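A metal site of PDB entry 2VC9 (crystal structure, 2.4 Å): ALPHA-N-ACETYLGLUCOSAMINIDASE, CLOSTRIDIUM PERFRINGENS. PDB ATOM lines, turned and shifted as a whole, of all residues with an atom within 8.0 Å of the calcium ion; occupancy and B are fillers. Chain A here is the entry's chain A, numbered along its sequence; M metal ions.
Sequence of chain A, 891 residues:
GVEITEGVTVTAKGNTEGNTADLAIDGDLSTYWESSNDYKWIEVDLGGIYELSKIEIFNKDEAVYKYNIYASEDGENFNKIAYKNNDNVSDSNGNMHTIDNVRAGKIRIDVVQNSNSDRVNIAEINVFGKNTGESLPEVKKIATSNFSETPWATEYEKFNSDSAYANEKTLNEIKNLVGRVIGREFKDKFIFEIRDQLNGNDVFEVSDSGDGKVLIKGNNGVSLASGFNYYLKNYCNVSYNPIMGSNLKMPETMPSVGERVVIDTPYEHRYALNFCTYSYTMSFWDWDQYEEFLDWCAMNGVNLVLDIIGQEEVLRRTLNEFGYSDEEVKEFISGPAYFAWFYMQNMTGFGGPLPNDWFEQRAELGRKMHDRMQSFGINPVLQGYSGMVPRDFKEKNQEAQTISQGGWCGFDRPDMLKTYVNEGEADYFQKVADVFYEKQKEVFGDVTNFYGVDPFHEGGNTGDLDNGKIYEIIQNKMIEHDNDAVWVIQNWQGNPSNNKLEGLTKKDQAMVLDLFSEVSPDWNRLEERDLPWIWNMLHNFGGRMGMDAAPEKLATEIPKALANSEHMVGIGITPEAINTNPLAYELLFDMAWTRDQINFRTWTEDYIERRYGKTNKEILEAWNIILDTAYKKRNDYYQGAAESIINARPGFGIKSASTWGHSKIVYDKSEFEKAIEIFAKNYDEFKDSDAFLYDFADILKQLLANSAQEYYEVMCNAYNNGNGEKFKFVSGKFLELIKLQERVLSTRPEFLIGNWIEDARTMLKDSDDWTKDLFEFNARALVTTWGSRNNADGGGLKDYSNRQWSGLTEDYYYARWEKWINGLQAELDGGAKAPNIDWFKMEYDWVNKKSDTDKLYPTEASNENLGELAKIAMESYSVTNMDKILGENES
Within 4 Å of the calcium ion: Leu 23, Asp 26, Asp 28, Thr 31, Ala 123 and Glu 124.
The side-chain carboxylate of Asp 28 sits at hydrogen-bond distance from the side-chain hydroxyl of Ser 30 (2.5 Å). The backbone NH (N) of Phe 58 lies within hydrogen-bond range of the backbone carbonyl oxygen (O) of Glu 124, at 2.8 Å. The backbone NH (N) of Gly 27 lies within hydrogen-bond range of the side-chain carboxylate (OE1) of Glu 124 (2.8 Å). The backbone NH (N) of Ala 123 sits at hydrogen-bond distance from the backbone carbonyl oxygen (O) of Phe 58 (2.9 Å).
The calcium ion is bound by the backbone carbonyl oxygen (O) of Leu 23, the backbone carbonyl oxygen (O) of Asp 28, the side-chain carboxylate (OD1) of Asp 26, the backbone carbonyl oxygen (O) of Thr 31, the backbone carbonyl oxygen (O) of Ala 123, the side-chain carboxylate (OE2) of Glu 124 and the side-chain hydroxyl (OG1) of Thr 31.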
ATOM      1  N   THR A  20      29.142  24.407  -6.591  1.00  0.00           N
ATOM      2  CA  THR A  20      29.554  24.583  -7.976  1.00  0.00           C
ATOM      3  C   THR A  20      29.793  23.247  -8.706  1.00  0.00           C
ATOM      4  O   THR A  20      30.066  22.227  -8.069  1.00  0.00           O
ATOM      5  CB  THR A  20      30.784  25.538  -8.045  1.00  0.00           C
ATOM      6  OG1 THR A  20      31.220  25.702  -9.406  1.00  0.00           O
ATOM      7  CG2 THR A  20      31.931  25.040  -7.173  1.00  0.00           C
ATOM      8  N   ALA A  21      29.650  23.263 -10.033  1.00  0.00           N
ATOM      9  CA  ALA A  21      29.678  22.041 -10.867  1.00  0.00           C
ATOM     10  C   ALA A  21      30.653  20.931 -10.421  1.00  0.00           C
ATOM     11  O   ALA A  21      30.243  19.783 -10.226  1.00  0.00           O
ATOM     12  CB  ALA A  21      29.910  22.414 -12.345  1.00  0.00           C
ATOM     13  N   ASP A  22      31.922  21.301 -10.253  1.00  0.00           N
ATOM     14  CA  ASP A  22      32.987  20.387  -9.793  1.00  0.00           C
ATOM     15  C   ASP A  22      32.701  19.649  -8.476  1.00  0.00           C
ATOM     16  O   ASP A  22      33.291  18.599  -8.210  1.00  0.00           O
ATOM     17  CB  ASP A  22      34.292  21.172  -9.639  1.00  0.00           C
ATOM     18  CG  ASP A  22      34.149  22.341  -8.706  1.00  0.00           C
ATOM     19  OD1 ASP A  22      34.750  22.324  -7.608  1.00  0.00           O
ATOM     20  OD2 ASP A  22      33.379  23.267  -9.041  1.00  0.00           O
ATOM     21  N   LEU A  23      31.810  20.193  -7.659  1.00  0.00           N
ATOM     22  CA  LEU A  23      31.440  19.557  -6.398  1.00  0.00           C
ATOM     23  C   LEU A  23      30.568  18.303  -6.596  1.00  0.00           C
ATOM     24  O   LEU A  23      30.376  17.517  -5.668  1.00  0.00           O
ATOM     25  CB  LEU A  23      30.770  20.554  -5.451  1.00  0.00           C
ATOM     26  CG  LEU A  23      31.585  21.712  -4.841  1.00  0.00           C
ATOM     27  CD1 LEU A  23      30.878  22.321  -3.631  1.00  0.00           C
ATOM     28  CD2 LEU A  23      33.014  21.300  -4.466  1.00  0.00           C
ATOM     29  N   ALA A  24      30.054  18.123  -7.810  1.00  0.00           N
ATOM     30  CA  ALA A  24      29.311  16.908  -8.155  1.00  0.00           C
ATOM     31  C   ALA A  24      30.248  15.737  -8.475  1.00  0.00           C
ATOM     32  O   ALA A  24      29.784  14.606  -8.653  1.00  0.00           O
ATOM     33  CB  ALA A  24      28.384  17.175  -9.338  1.00  0.00           C
ATOM     34  N   ILE A  25      31.547  16.020  -8.573  1.00  0.00           N
ATOM     35  CA  ILE A  25      32.536  15.015  -8.993  1.00  0.00           C
ATOM     36  C   ILE A  25      33.839  15.016  -8.155  1.00  0.00           C
ATOM     37  O   ILE A  25      34.901  14.604  -8.644  1.00  0.00           O
ATOM     38  CB  ILE A  25      32.884  15.165 -10.509  1.00  0.00           C
ATOM     39  CG1 ILE A  25      33.398  16.569 -10.822  1.00  0.00           C
ATOM     40  CG2 ILE A  25      31.695  14.809 -11.403  1.00  0.00           C
ATOM     41  CD1 ILE A  25      34.279  16.632 -12.049  1.00  0.00           C
ATOM     42  N   ASP A  26      33.783  15.448  -6.901  1.00  0.00           N
ATOM     43  CA  ASP A  26      34.995  15.536  -6.066  1.00  0.00           C
ATOM     44  C   ASP A  26      35.249  14.309  -5.156  1.00  0.00           C
ATOM     45  O   ASP A  26      36.149  14.326  -4.327  1.00  0.00           O
ATOM     46  CB  ASP A  26      35.061  16.847  -5.266  1.00  0.00           C
ATOM     47  CG  ASP A  26      33.848  17.077  -4.383  1.00  0.00           C
ATOM     48  OD1 ASP A  26      32.927  16.221  -4.379  1.00  0.00           O
ATOM     49  OD2 ASP A  26      33.791  18.103  -3.695  1.00  0.00           O
ATOM     50  N   GLY A  27      34.478  13.235  -5.350  1.00  0.00           N
ATOM     51  CA  GLY A  27      34.574  12.037  -4.510  1.00  0.00           C
ATOM     52  C   GLY A  27      34.059  12.241  -3.085  1.00  0.00           C
ATOM     53  O   GLY A  27      34.335  11.435  -2.215  1.00  0.00           O
ATOM     54  N   ASP A  28      33.303  13.318  -2.864  1.00  0.00           N
ATOM     55  CA  ASP A  28      32.917  13.756  -1.543  1.00  0.00           C
ATOM     56  C   ASP A  28      31.405  13.895  -1.464  1.00  0.00           C
ATOM     57  O   ASP A  28      30.815  14.746  -2.124  1.00  0.00           O
ATOM     58  CB  ASP A  28      33.603  15.084  -1.223  1.00  0.00           C
ATOM     59  CG  ASP A  28      33.475  15.507   0.232  1.00  0.00           C
ATOM     60  OD1 ASP A  28      32.635  14.946   0.970  1.00  0.00           O
ATOM     61  OD2 ASP A  28      34.210  16.428   0.647  1.00  0.00           O
ATOM     62  N   LEU A  29      30.778  13.042  -0.650  1.00  0.00           N
ATOM     63  CA  LEU A  29      29.318  13.018  -0.496  1.00  0.00           C
ATOM     64  C   LEU A  29      28.742  14.204   0.275  1.00  0.00           C
ATOM     65  O   LEU A  29      27.534  14.412   0.289  1.00  0.00           O
ATOM     66  CB  LEU A  29      28.888  11.710   0.171  1.00  0.00           C
ATOM     67  CG  LEU A  29      28.281  10.583  -0.678  1.00  0.00           C
ATOM     68  CD1 LEU A  29      28.795  10.506  -2.090  1.00  0.00           C
ATOM     69  CD2 LEU A  29      28.508   9.302   0.033  1.00  0.00           C
ATOM     70  N   SER A  30      29.619  14.983   0.913  1.00  0.00           N
ATOM     71  CA  SER A  30      29.174  16.098   1.750  1.00  0.00           C
ATOM     72  C   SER A  30      29.132  17.401   0.959  1.00  0.00           C
ATOM     73  O   SER A  30      28.511  18.370   1.390  1.00  0.00           O
ATOM     74  CB  SER A  30      30.074  16.249   2.985  1.00  0.00           C
ATOM     75  OG  SER A  30      31.418  16.440   2.596  1.00  0.00           O
ATOM     76  N   THR A  31      29.793  17.428  -0.194  1.00  0.00           N
ATOM     77  CA  THR A  31      29.778  18.582  -1.078  1.00  0.00           C
ATOM     78  C   THR A  31      28.893  18.268  -2.286  1.00  0.00           C
ATOM     79  O   THR A  31      28.839  17.112  -2.726  1.00  0.00           O
ATOM     80  CB  THR A  31      31.191  18.979  -1.557  1.00  0.00           C
ATOM     81  OG1 THR A  31      31.759  17.927  -2.349  1.00  0.00           O
ATOM     82  CG2 THR A  31      32.100  19.284  -0.376  1.00  0.00           C
ATOM     83  N   TYR A  32      28.220  19.280  -2.818  1.00  0.00           N
ATOM     84  CA  TYR A  32      27.290  19.069  -3.938  1.00  0.00           C
ATOM     85  C   TYR A  32      27.183  20.261  -4.892  1.00  0.00           C
ATOM     86  O   TYR A  32      27.348  21.413  -4.480  1.00  0.00           O
ATOM     87  CB  TYR A  32      25.912  18.716  -3.386  1.00  0.00           C
ATOM     88  CG  TYR A  32      25.329  19.766  -2.466  1.00  0.00           C
ATOM     89  CD1 TYR A  32      25.482  19.666  -1.087  1.00  0.00           C
ATOM     90  CD2 TYR A  32      24.632  20.869  -2.980  1.00  0.00           C
ATOM     91  CE1 TYR A  32      24.951  20.636  -0.233  1.00  0.00           C
ATOM     92  CE2 TYR A  32      24.103  21.844  -2.135  1.00  0.00           C
ATOM     93  CZ  TYR A  32      24.269  21.711  -0.767  1.00  0.00           C
ATOM     94  OH  TYR A  32      23.745  22.669   0.092  1.00  0.00           O
ATOM     95  N   TRP A  33      26.921  19.989  -6.172  1.00  0.00           N
ATOM     96  CA  TRP A  33      26.417  21.009  -7.080  1.00  0.00           C
ATOM     97  C   TRP A  33      24.927  21.236  -6.763  1.00  0.00           C
ATOM     98  O   TRP A  33      24.221  20.305  -6.421  1.00  0.00           O
ATOM     99  CB  TRP A  33      26.589  20.607  -8.559  1.00  0.00           C
ATOM    100  CG  TRP A  33      25.716  21.421  -9.507  1.00  0.00           C
ATOM    101  CD1 TRP A  33      25.967  22.678  -9.958  1.00  0.00           C
ATOM    102  CD2 TRP A  33      24.443  21.037 -10.062  1.00  0.00           C
ATOM    103  NE1 TRP A  33      24.943  23.099 -10.782  1.00  0.00           N
ATOM    104  CE2 TRP A  33      23.992  22.112 -10.856  1.00  0.00           C
ATOM    105  CE3 TRP A  33      23.645  19.876  -9.976  1.00  0.00           C
ATOM    106  CZ2 TRP A  33      22.778  22.081 -11.564  1.00  0.00           C
ATOM    107  CZ3 TRP A  33      22.431  19.845 -10.684  1.00  0.00           C
ATOM    108  CH2 TRP A  33      22.009  20.938 -11.456  1.00  0.00           C
ATOM    109  N   PHE A  58      24.296  10.179  -6.344  1.00  0.00           N
ATOM    110  CA  PHE A  58      23.938  10.523  -4.974  1.00  0.00           C
ATOM    111  C   PHE A  58      23.407  11.949  -4.949  1.00  0.00           C
ATOM    112  O   PHE A  58      23.888  12.817  -5.667  1.00  0.00           O
ATOM    113  CB  PHE A  58      25.157  10.444  -4.039  1.00  0.00           C
ATOM    114  CG  PHE A  58      25.735   9.052  -3.878  1.00  0.00           C
ATOM    115  CD1 PHE A  58      25.388   8.270  -2.773  1.00  0.00           C
ATOM    116  CD2 PHE A  58      26.629   8.543  -4.810  1.00  0.00           C
ATOM    117  CE1 PHE A  58      25.926   6.991  -2.620  1.00  0.00           C
ATOM    118  CE2 PHE A  58      27.174   7.277  -4.658  1.00  0.00           C
ATOM    119  CZ  PHE A  58      26.820   6.496  -3.581  1.00  0.00           C
ATOM    120  N   ILE A 122      23.229  17.441  -7.191  1.00  0.00           N
ATOM    121  CA  ILE A 122      23.907  16.154  -7.262  1.00  0.00           C
ATOM    122  C   ILE A 122      25.126  16.231  -6.328  1.00  0.00           C
ATOM    123  O   ILE A 122      26.015  17.061  -6.522  1.00  0.00           O
ATOM    124  CB  ILE A 122      24.332  15.795  -8.707  1.00  0.00           C
ATOM    125  CG1 ILE A 122      23.107  15.682  -9.620  1.00  0.00           C
ATOM    126  CG2 ILE A 122      25.111  14.460  -8.739  1.00  0.00           C
ATOM    127  CD1 ILE A 122      23.356  16.041 -11.052  1.00  0.00           C
ATOM    128  N   ALA A 123      25.137  15.377  -5.300  1.00  0.00           N
ATOM    129  CA  ALA A 123      26.266  15.327  -4.363  1.00  0.00           C
ATOM    130  C   ALA A 123      27.463  14.606  -4.984  1.00  0.00           C
ATOM    131  O   ALA A 123      28.591  15.070  -4.879  1.00  0.00           O
ATOM    132  CB  ALA A 123      25.863  14.668  -3.036  1.00  0.00           C
ATOM    133  N   GLU A 124      27.208  13.466  -5.621  1.00  0.00           N
ATOM    134  CA  GLU A 124      28.242  12.754  -6.370  1.00  0.00           C
ATOM    135  C   GLU A 124      27.630  12.008  -7.538  1.00  0.00           C
ATOM    136  O   GLU A 124      26.473  11.580  -7.474  1.00  0.00           O
ATOM    137  CB  GLU A 124      28.986  11.738  -5.478  1.00  0.00           C
ATOM    138  CG  GLU A 124      30.141  12.280  -4.648  1.00  0.00           C
ATOM    139  CD  GLU A 124      31.199  12.975  -5.471  1.00  0.00           C
ATOM    140  OE1 GLU A 124      31.963  12.279  -6.182  1.00  0.00           O
ATOM    141  OE2 GLU A 124      31.277  14.216  -5.406  1.00  0.00           O
ATOM    142  N   ILE A 125      28.411  11.876  -8.595  1.00  0.00           N
ATOM    143  CA  ILE A 125      28.105  10.973  -9.699  1.00  0.00           C
ATOM    144  C   ILE A 125      29.360  10.198 -10.111  1.00  0.00           C
ATOM    145  O   ILE A 125      30.387  10.786 -10.487  1.00  0.00           O
ATOM    146  CB  ILE A 125      27.458  11.699 -10.904  1.00  0.00           C
ATOM    147  CG1 ILE A 125      27.044  10.665 -11.971  1.00  0.00           C
ATOM    148  CG2 ILE A 125      28.382  12.800 -11.460  1.00  0.00           C
ATOM    149  CD1 ILE A 125      26.584  11.252 -13.285  1.00  0.00           C
HETATM  150 CA    CA M   1      30.611  16.107  -3.959  1.00  0.00          CA
